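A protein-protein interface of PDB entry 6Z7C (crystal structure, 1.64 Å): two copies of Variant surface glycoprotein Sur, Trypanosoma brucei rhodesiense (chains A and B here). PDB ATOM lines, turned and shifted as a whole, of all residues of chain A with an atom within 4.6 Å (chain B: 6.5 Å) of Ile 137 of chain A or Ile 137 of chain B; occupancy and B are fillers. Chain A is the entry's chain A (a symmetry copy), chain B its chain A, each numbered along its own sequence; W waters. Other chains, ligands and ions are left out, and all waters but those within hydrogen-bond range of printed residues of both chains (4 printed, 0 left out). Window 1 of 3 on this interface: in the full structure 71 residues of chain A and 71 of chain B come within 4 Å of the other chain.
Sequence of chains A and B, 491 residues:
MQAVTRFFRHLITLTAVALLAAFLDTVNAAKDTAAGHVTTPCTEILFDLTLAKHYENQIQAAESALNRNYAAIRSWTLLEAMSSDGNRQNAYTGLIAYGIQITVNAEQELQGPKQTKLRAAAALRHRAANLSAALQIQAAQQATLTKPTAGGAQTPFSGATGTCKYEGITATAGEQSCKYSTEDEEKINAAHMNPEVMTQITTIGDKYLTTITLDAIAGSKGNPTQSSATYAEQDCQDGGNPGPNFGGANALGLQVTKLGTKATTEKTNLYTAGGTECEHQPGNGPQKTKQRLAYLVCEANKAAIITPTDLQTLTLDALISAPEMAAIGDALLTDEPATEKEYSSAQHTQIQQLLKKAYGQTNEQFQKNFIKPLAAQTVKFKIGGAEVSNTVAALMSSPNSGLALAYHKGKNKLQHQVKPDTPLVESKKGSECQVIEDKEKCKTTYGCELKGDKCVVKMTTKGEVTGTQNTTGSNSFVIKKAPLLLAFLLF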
ATOM      1  N   ALA A 133      30.171  -3.768  30.998  1.00  0.00           N
ATOM      2  CA  ALA A 133      30.188  -2.441  30.395  1.00  0.00           C
ATOM      3  C   ALA A 133      28.793  -2.043  29.942  1.00  0.00           C
ATOM      4  O   ALA A 133      28.368  -0.894  30.135  1.00  0.00           O
ATOM      5  CB  ALA A 133      31.176  -2.406  29.221  1.00  0.00           C
ATOM      6  N   ALA A 134      28.063  -2.982  29.340  1.00  0.00           N
ATOM      7  CA  ALA A 134      26.687  -2.704  28.950  1.00  0.00           C
ATOM      8  C   ALA A 134      25.824  -2.412  30.167  1.00  0.00           C
ATOM      9  O   ALA A 134      24.966  -1.518  30.130  1.00  0.00           O
ATOM     10  CB  ALA A 134      26.129  -3.884  28.154  1.00  0.00           C
ATOM     11  N   LEU A 135      26.027  -3.166  31.249  1.00  0.00           N
ATOM     12  CA  LEU A 135      25.292  -2.929  32.490  1.00  0.00           C
ATOM     13  C   LEU A 135      25.472  -1.493  32.977  1.00  0.00           C
ATOM     14  O   LEU A 135      24.508  -0.849  33.418  1.00  0.00           O
ATOM     15  CB  LEU A 135      25.754  -3.928  33.551  1.00  0.00           C
ATOM     16  CG  LEU A 135      25.051  -3.985  34.911  1.00  0.00           C
ATOM     17  CD1 LEU A 135      25.299  -5.342  35.551  1.00  0.00           C
ATOM     18  CD2 LEU A 135      25.548  -2.911  35.841  1.00  0.00           C
ATOM     19  N   GLN A 136      26.702  -0.979  32.936  1.00  0.00           N
ATOM     20  CA  GLN A 136      26.938   0.388  33.396  1.00  0.00           C
ATOM     21  C   GLN A 136      26.155   1.393  32.557  1.00  0.00           C
ATOM     22  O   GLN A 136      25.549   2.331  33.093  1.00  0.00           O
ATOM     23  CB  GLN A 136      28.433   0.696  33.363  1.00  0.00           C
ATOM     24  CG  GLN A 136      28.775   2.137  33.760  1.00  0.00           C
ATOM     25  CD  GLN A 136      28.486   2.402  35.224  1.00  0.00           C
ATOM     26  OE1 GLN A 136      28.840   1.599  36.086  1.00  0.00           O
ATOM     27  NE2 GLN A 136      27.845   3.523  35.513  1.00  0.00           N
ATOM     28  N   ILE A 137      26.134   1.198  31.238  1.00  0.00           N
ATOM     29  CA  ILE A 137      25.410   2.111  30.361  1.00  0.00           C
ATOM     30  C   ILE A 137      23.899   1.941  30.517  1.00  0.00           C
ATOM     31  O   ILE A 137      23.152   2.927  30.532  1.00  0.00           O
ATOM     32  CB  ILE A 137      25.878   1.899  28.912  1.00  0.00           C
ATOM     33  CG1 ILE A 137      27.346   2.331  28.798  1.00  0.00           C
ATOM     34  CG2 ILE A 137      24.987   2.673  27.934  1.00  0.00           C
ATOM     35  CD1 ILE A 137      27.983   2.049  27.437  1.00  0.00           C
ATOM     36  N   GLN A 138      23.417   0.698  30.656  1.00  0.00           N
ATOM     37  CA  GLN A 138      21.971   0.522  30.778  1.00  0.00           C
ATOM     38  C   GLN A 138      21.441   1.005  32.124  1.00  0.00           C
ATOM     39  O   GLN A 138      20.223   1.175  32.278  1.00  0.00           O
ATOM     40  CB  GLN A 138      21.582  -0.950  30.538  1.00  0.00           C
ATOM     41  CG  GLN A 138      21.917  -1.494  29.123  1.00  0.00           C
ATOM     42  CD  GLN A 138      21.142  -0.803  27.994  1.00  0.00           C
ATOM     43  OE1 GLN A 138      20.254   0.021  28.236  1.00  0.00           O
ATOM     44  NE2 GLN A 138      21.473  -1.150  26.757  1.00  0.00           N
ATOM     45  N   ALA A 139      22.321   1.271  33.086  1.00  0.00           N
ATOM     46  CA  ALA A 139      21.921   1.859  34.357  1.00  0.00           C
ATOM     47  C   ALA A 139      21.710   3.369  34.276  1.00  0.00           C
ATOM     48  O   ALA A 139      21.208   3.969  35.240  1.00  0.00           O
ATOM     49  CB  ALA A 139      22.984   1.552  35.417  1.00  0.00           C
ATOM     50  N   ALA A 140      22.116   4.003  33.174  1.00  0.00           N
ATOM     51  CA  ALA A 140      21.957   5.448  33.013  1.00  0.00           C
ATOM     52  C   ALA A 140      20.523   5.697  32.589  1.00  0.00           C
ATOM     53  O   ALA A 140      20.201   5.759  31.396  1.00  0.00           O
ATOM     54  CB  ALA A 140      22.948   6.001  31.998  1.00  0.00           C
ATOM     55  N   LEU A 209      23.089  -5.270  24.887  1.00  0.00           N
ATOM     56  CA  LEU A 209      24.419  -4.827  24.510  1.00  0.00           C
ATOM     57  C   LEU A 209      24.435  -3.894  23.305  1.00  0.00           C
ATOM     58  O   LEU A 209      25.486  -3.314  23.008  1.00  0.00           O
ATOM     59  CB  LEU A 209      25.309  -6.048  24.240  1.00  0.00           C
ATOM     60  CG  LEU A 209      25.587  -6.778  25.562  1.00  0.00           C
ATOM     61  CD1 LEU A 209      24.700  -8.003  25.732  1.00  0.00           C
ATOM     62  CD2 LEU A 209      27.062  -7.112  25.767  1.00  0.00           C
ATOM     63  N   THR A 210      23.314  -3.714  22.610  1.00  0.00           N
ATOM     64  CA  THR A 210      23.320  -2.936  21.377  1.00  0.00           C
ATOM     65  C   THR A 210      22.369  -1.752  21.357  1.00  0.00           C
ATOM     66  O   THR A 210      22.534  -0.880  20.498  1.00  0.00           O
ATOM     67  CB  THR A 210      22.956  -3.818  20.175  1.00  0.00           C
ATOM     68  OG1 THR A 210      21.579  -4.212  20.296  1.00  0.00           O
ATOM     69  CG2 THR A 210      23.841  -5.056  20.128  1.00  0.00           C
ATOM     70  N   ILE A 212      19.866   1.410  22.845  1.00  0.00           N
ATOM     71  CA  ILE A 212      19.439   2.430  23.797  1.00  0.00           C
ATOM     72  C   ILE A 212      17.923   2.550  23.693  1.00  0.00           C
ATOM     73  O   ILE A 212      17.377   2.593  22.585  1.00  0.00           O
ATOM     74  CB  ILE A 212      20.120   3.778  23.504  1.00  0.00           C
ATOM     75  CG1 ILE A 212      21.626   3.699  23.765  1.00  0.00           C
ATOM     76  CG2 ILE A 212      19.469   4.909  24.322  1.00  0.00           C
ATOM     77  CD1 ILE A 212      22.386   4.863  23.155  1.00  0.00           C
ATOM     78  N   SER B 132      35.260  -1.859  23.331  1.00  0.00           N
ATOM     79  CA  SER B 132      34.572  -2.365  22.148  1.00  0.00           C
ATOM     80  C   SER B 132      33.063  -2.404  22.362  1.00  0.00           C
ATOM     81  O   SER B 132      32.290  -2.107  21.440  1.00  0.00           O
ATOM     82  CB  SER B 132      35.098  -3.755  21.794  1.00  0.00           C
ATOM     83  OG  SER B 132      34.562  -4.755  22.644  1.00  0.00           O
ATOM     84  N   ALA B 133      32.625  -2.781  23.570  1.00  0.00           N
ATOM     85  CA  ALA B 133      31.202  -2.817  23.880  1.00  0.00           C
ATOM     86  C   ALA B 133      30.629  -1.409  23.922  1.00  0.00           C
ATOM     87  O   ALA B 133      29.528  -1.157  23.411  1.00  0.00           O
ATOM     88  CB  ALA B 133      30.967  -3.544  25.211  1.00  0.00           C
ATOM     89  N   ALA B 134      31.366  -0.477  24.526  1.00  0.00           N
ATOM     90  CA  ALA B 134      30.926   0.912  24.537  1.00  0.00           C
ATOM     91  C   ALA B 134      30.859   1.474  23.126  1.00  0.00           C
ATOM     92  O   ALA B 134      29.929   2.222  22.790  1.00  0.00           O
ATOM     93  CB  ALA B 134      31.865   1.742  25.413  1.00  0.00           C
ATOM     94  N   LEU B 135      31.844   1.137  22.292  1.00  0.00           N
ATOM     95  CA  LEU B 135      31.843   1.575  20.897  1.00  0.00           C
ATOM     96  C   LEU B 135      30.564   1.149  20.181  1.00  0.00           C
ATOM     97  O   LEU B 135      29.977   1.929  19.418  1.00  0.00           O
ATOM     98  CB  LEU B 135      33.078   1.017  20.191  1.00  0.00           C
ATOM     99  CG  LEU B 135      33.392   1.431  18.749  1.00  0.00           C
ATOM    100  CD1 LEU B 135      34.870   1.205  18.469  1.00  0.00           C
ATOM    101  CD2 LEU B 135      32.582   0.645  17.754  1.00  0.00           C
ATOM    102  N   GLN B 136      30.129  -0.095  20.389  1.00  0.00           N
ATOM    103  CA  GLN B 136      28.914  -0.564  19.724  1.00  0.00           C
ATOM    104  C   GLN B 136      27.704   0.262  20.147  1.00  0.00           C
ATOM    105  O   GLN B 136      26.873   0.643  19.312  1.00  0.00           O
ATOM    106  CB  GLN B 136      28.698  -2.045  20.024  1.00  0.00           C
ATOM    107  CG  GLN B 136      27.404  -2.612  19.429  1.00  0.00           C
ATOM    108  CD  GLN B 136      27.451  -2.655  17.914  1.00  0.00           C
ATOM    109  OE1 GLN B 136      28.445  -3.090  17.333  1.00  0.00           O
ATOM    110  NE2 GLN B 136      26.385  -2.210  17.269  1.00  0.00           N
ATOM    111  N   ILE B 137      27.601   0.570  21.441  1.00  0.00           N
ATOM    112  CA  ILE B 137      26.474   1.356  21.932  1.00  0.00           C
ATOM    113  C   ILE B 137      26.583   2.813  21.484  1.00  0.00           C
ATOM    114  O   ILE B 137      25.581   3.433  21.105  1.00  0.00           O
ATOM    115  CB  ILE B 137      26.388   1.218  23.461  1.00  0.00           C
ATOM    116  CG1 ILE B 137      26.032  -0.235  23.806  1.00  0.00           C
ATOM    117  CG2 ILE B 137      25.365   2.201  24.040  1.00  0.00           C
ATOM    118  CD1 ILE B 137      26.043  -0.549  25.302  1.00  0.00           C
ATOM    119  N   GLN B 138      27.794   3.387  21.497  1.00  0.00           N
ATOM    120  CA  GLN B 138      27.905   4.789  21.097  1.00  0.00           C
ATOM    121  C   GLN B 138      27.701   4.980  19.598  1.00  0.00           C
ATOM    122  O   GLN B 138      27.496   6.116  19.147  1.00  0.00           O
ATOM    123  CB  GLN B 138      29.261   5.373  21.538  1.00  0.00           C
ATOM    124  CG  GLN B 138      29.499   5.392  23.073  1.00  0.00           C
ATOM    125  CD  GLN B 138      28.530   6.301  23.838  1.00  0.00           C
ATOM    126  OE1 GLN B 138      27.727   7.029  23.244  1.00  0.00           O
ATOM    127  NE2 GLN B 138      28.614   6.267  25.162  1.00  0.00           N
ATOM    128  N   ALA B 139      27.708   3.899  18.820  1.00  0.00           N
ATOM    129  CA  ALA B 139      27.392   3.969  17.400  1.00  0.00           C
ATOM    130  C   ALA B 139      25.892   4.030  17.125  1.00  0.00           C
ATOM    131  O   ALA B 139      25.490   4.259  15.972  1.00  0.00           O
ATOM    132  CB  ALA B 139      27.990   2.751  16.686  1.00  0.00           C
ATOM    133  N   ALA B 140      25.055   3.790  18.137  1.00  0.00           N
ATOM    134  CA  ALA B 140      23.604   3.824  17.962  1.00  0.00           C
ATOM    135  C   ALA B 140      23.181   5.279  17.999  1.00  0.00           C
ATOM    136  O   ALA B 140      22.837   5.828  19.053  1.00  0.00           O
ATOM    137  CB  ALA B 140      22.901   3.006  19.037  1.00  0.00           C
ATOM    138  N   GLN B 141      23.224   5.919  16.834  1.00  0.00           N
ATOM    139  CA  GLN B 141      23.106   7.365  16.759  1.00  0.00           C
ATOM    140  C   GLN B 141      21.849   7.831  16.048  1.00  0.00           C
ATOM    141  O   GLN B 141      21.625   9.046  15.950  1.00  0.00           O
ATOM    142  CB  GLN B 141      24.346   7.945  16.071  1.00  0.00           C
ATOM    143  CG  GLN B 141      25.605   7.590  16.844  1.00  0.00           C
ATOM    144  CD  GLN B 141      26.793   8.403  16.415  1.00  0.00           C
ATOM    145  OE1 GLN B 141      26.725   9.152  15.444  1.00  0.00           O
ATOM    146  NE2 GLN B 141      27.897   8.270  17.146  1.00  0.00           N
ATOM    147  N   ALA B 171      17.430   3.234  19.836  1.00  0.00           N
ATOM    148  CA  ALA B 171      18.516   3.457  18.893  1.00  0.00           C
ATOM    149  C   ALA B 171      19.408   2.229  18.912  1.00  0.00           C
ATOM    150  O   ALA B 171      19.794   1.765  19.990  1.00  0.00           O
ATOM    151  CB  ALA B 171      19.326   4.709  19.243  1.00  0.00           C
ATOM    152  N   ALA B 173      22.684   0.315  16.412  1.00  0.00           N
ATOM    153  CA  ALA B 173      23.565   0.362  15.256  1.00  0.00           C
ATOM    154  C   ALA B 173      23.788  -1.046  14.722  1.00  0.00           C
ATOM    155  O   ALA B 173      23.685  -2.028  15.459  1.00  0.00           O
ATOM    156  CB  ALA B 173      24.910   0.994  15.606  1.00  0.00           C
ATOM    157  N   GLN B 176      29.415  -3.064  14.581  1.00  0.00           N
ATOM    158  CA  GLN B 176      30.578  -2.212  14.369  1.00  0.00           C
ATOM    159  C   GLN B 176      31.845  -3.050  14.334  1.00  0.00           C
ATOM    160  O   GLN B 176      31.938  -4.093  14.982  1.00  0.00           O
ATOM    161  CB  GLN B 176      30.689  -1.165  15.479  1.00  0.00           C
ATOM    162  CG  GLN B 176      29.462  -0.272  15.574  1.00  0.00           C
ATOM    163  CD  GLN B 176      29.276   0.561  14.319  1.00  0.00           C
ATOM    164  OE1 GLN B 176      30.121   1.390  13.987  1.00  0.00           O
ATOM    165  NE2 GLN B 176      28.186   0.324  13.602  1.00  0.00           N
ATOM    166  N   TYR B 208      32.761   8.165  27.617  1.00  0.00           N
ATOM    167  CA  TYR B 208      32.435   7.294  26.490  1.00  0.00           C
ATOM    168  C   TYR B 208      31.881   5.958  26.962  1.00  0.00           C
ATOM    169  O   TYR B 208      31.059   5.338  26.272  1.00  0.00           O
ATOM    170  CB  TYR B 208      33.683   7.078  25.643  1.00  0.00           C
ATOM    171  CG  TYR B 208      33.434   6.492  24.282  1.00  0.00           C
ATOM    172  CD1 TYR B 208      32.925   7.276  23.240  1.00  0.00           C
ATOM    173  CD2 TYR B 208      33.740   5.160  24.019  1.00  0.00           C
ATOM    174  CE1 TYR B 208      32.722   6.735  21.977  1.00  0.00           C
ATOM    175  CE2 TYR B 208      33.539   4.611  22.756  1.00  0.00           C
ATOM    176  CZ  TYR B 208      33.036   5.409  21.744  1.00  0.00           C
ATOM    177  OH  TYR B 208      32.841   4.877  20.499  1.00  0.00           O
ATOM    178  N   LEU B 209      32.308   5.513  28.139  1.00  0.00           N
ATOM    179  CA  LEU B 209      31.875   4.247  28.702  1.00  0.00           C
ATOM    180  C   LEU B 209      30.701   4.376  29.666  1.00  0.00           C
ATOM    181  O   LEU B 209      30.134   3.352  30.064  1.00  0.00           O
ATOM    182  CB  LEU B 209      33.057   3.565  29.405  1.00  0.00           C
ATOM    183  CG  LEU B 209      34.076   3.104  28.352  1.00  0.00           C
ATOM    184  CD1 LEU B 209      35.253   4.063  28.243  1.00  0.00           C
ATOM    185  CD2 LEU B 209      34.536   1.663  28.551  1.00  0.00           C
ATOM    186  N   THR B 210      30.304   5.589  30.045  1.00  0.00           N
ATOM    187  CA  THR B 210      29.274   5.750  31.064  1.00  0.00           C
ATOM    188  C   THR B 210      28.061   6.555  30.633  1.00  0.00           C
ATOM    189  O   THR B 210      27.031   6.475  31.312  1.00  0.00           O
ATOM    190  CB  THR B 210      29.846   6.443  32.309  1.00  0.00           C
ATOM    191  OG1 THR B 210      30.173   7.801  31.970  1.00  0.00           O
ATOM    192  CG2 THR B 210      31.094   5.723  32.801  1.00  0.00           C
ATOM    193  N   THR B 211      28.148   7.347  29.569  1.00  0.00           N
ATOM    194  CA  THR B 211      27.184   8.416  29.350  1.00  0.00           C
ATOM    195  C   THR B 211      26.492   8.257  28.005  1.00  0.00           C
ATOM    196  O   THR B 211      27.151   8.046  26.981  1.00  0.00           O
ATOM    197  CB  THR B 211      27.879   9.777  29.440  1.00  0.00           C
ATOM    198  OG1 THR B 211      28.395   9.956  30.764  1.00  0.00           O
ATOM    199  CG2 THR B 211      26.924  10.907  29.124  1.00  0.00           C
ATOM    200  N   ILE B 212      25.160   8.352  28.019  1.00  0.00           N
ATOM    201  CA  ILE B 212      24.352   8.466  26.809  1.00  0.00           C
ATOM    202  C   ILE B 212      24.121   9.950  26.549  1.00  0.00           C
ATOM    203  O   ILE B 212      23.800  10.702  27.477  1.00  0.00           O
ATOM    204  CB  ILE B 212      23.016   7.719  26.966  1.00  0.00           C
ATOM    205  CG1 ILE B 212      23.242   6.209  27.066  1.00  0.00           C
ATOM    206  CG2 ILE B 212      22.056   8.066  25.812  1.00  0.00           C
ATOM    207  CD1 ILE B 212      22.020   5.469  27.579  1.00  0.00           C
ATOM    208  N   GLY B 260      24.735   9.720  20.732  1.00  0.00           N
ATOM    209  CA  GLY B 260      26.162   9.379  20.660  1.00  0.00           C
ATOM    210  C   GLY B 260      27.006  10.345  21.464  1.00  0.00           C
ATOM    211  O   GLY B 260      26.893  11.571  21.357  1.00  0.00           O
HETATM  212  O   HOH W   1      26.358   5.007  33.350  1.00  0.00           O
HETATM  213  O   HOH W   2      28.022  -3.568  23.632  1.00  0.00           O
HETATM  214  O   HOH W   3      30.672   0.784  30.080  1.00  0.00           O
HETATM  215  O   HOH W   4      24.373  -0.481  18.703  1.00  0.00           O
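Water W1 lies within hydrogen-bond range of the backbone carbonyl oxygen of Thr 210 of chain B and the backbone carbonyl oxygen of Gln 136 of chain A. Water W4 lies within hydrogen-bond range of O of Thr 210 of chain A, O of Gln 136 of chain B and N of Ala 173 of chain B. Water W3 bridges O of Leu 209 of chain B (2.6 Å) and O of Ala 133 of chain A (2.9 Å). Water W2 bridges the backbone carbonyl oxygen of Leu 209 of chain A (2.6 Å) and the backbone carbonyl oxygen of Ala 133 of chain B (2.9 Å).
Of the 11 printed residues of chain A, 4 touch a printed residue of chain B. Hydrophobic or aromatic side chains of chain A within 4 Å of the printed part of chain B: Ile 137. Of the 19 printed residues of chain B, 3 touch a printed residue of chain A. Printed residues of chain B that touch a printed residue of chain A: Ile 137, Ala 171 and Leu 209. Hydrophobic or aromatic side chains of chain B that line the printed part of chain A: Ile 137. Among the printed residues, 5 pairs touch across the chains. Among the printed residues, no Asp or Glu carboxylate lies within 4 Å of a Lys or Arg side-chain nitrogen of the other chain.
Ile 137 of chain B touches its own counterpart, Ile 137 of chain A. Ile 137 of chain A touches Leu 209 of chain B, and with the chains exchanged Leu 209 of chain A touches Ile 137 of chain B. Positions printed for both chains: 133, 134, 135, 136, 137, 138, 139, 140, 209, 210 and 212. Of the 5 pairs that touch across the chains among the printed residues, 3 have their exchanged pair printed and touching as well.
Of chain A, only Ile 137 (3.9 Å) and Leu 209 (3.2 Å) come within 4 Å of Ile 137 of chain B. Of the printed residues of chain A, Leu 209 of chain B touches Ile 137. Printed residues of chain B within 4 Å of Leu 209 of chain A: Ile 137. Of the printed residues of chain B, Thr 210 of chain A touches Ala 171. Printed residues of chain B within 4 Å of Ile 212 of chain A: Ala 171. Of the printed residues of chain A, Ala 171 of chain B touches Thr 210 (3.8 Å) and Ile 212 (2.8 Å). The nearest residue of chain A that does not touch Ile 137 of chain B is Ile 212 of chain A (4.04 Å). The nearest printed residue of chain A that does not touch Ala 171 of chain B is Gln 138 of chain A (7.6 Å).
Ile 137 of chain B touches Ile 137 of chain A (CD1 to CD1, 3.9 Å). Ile 137 of chain A touches Leu 209 of chain B. Ile 137 of chain B touches Leu 209 of chain A (CG1 to O, 3.2 Å). Ala 171 of chain B touches Thr 210 of chain A.
O of Ile 212 of chain A is in hydrogen-bond range of N of Ala 171 of chain B (2.8 Å).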
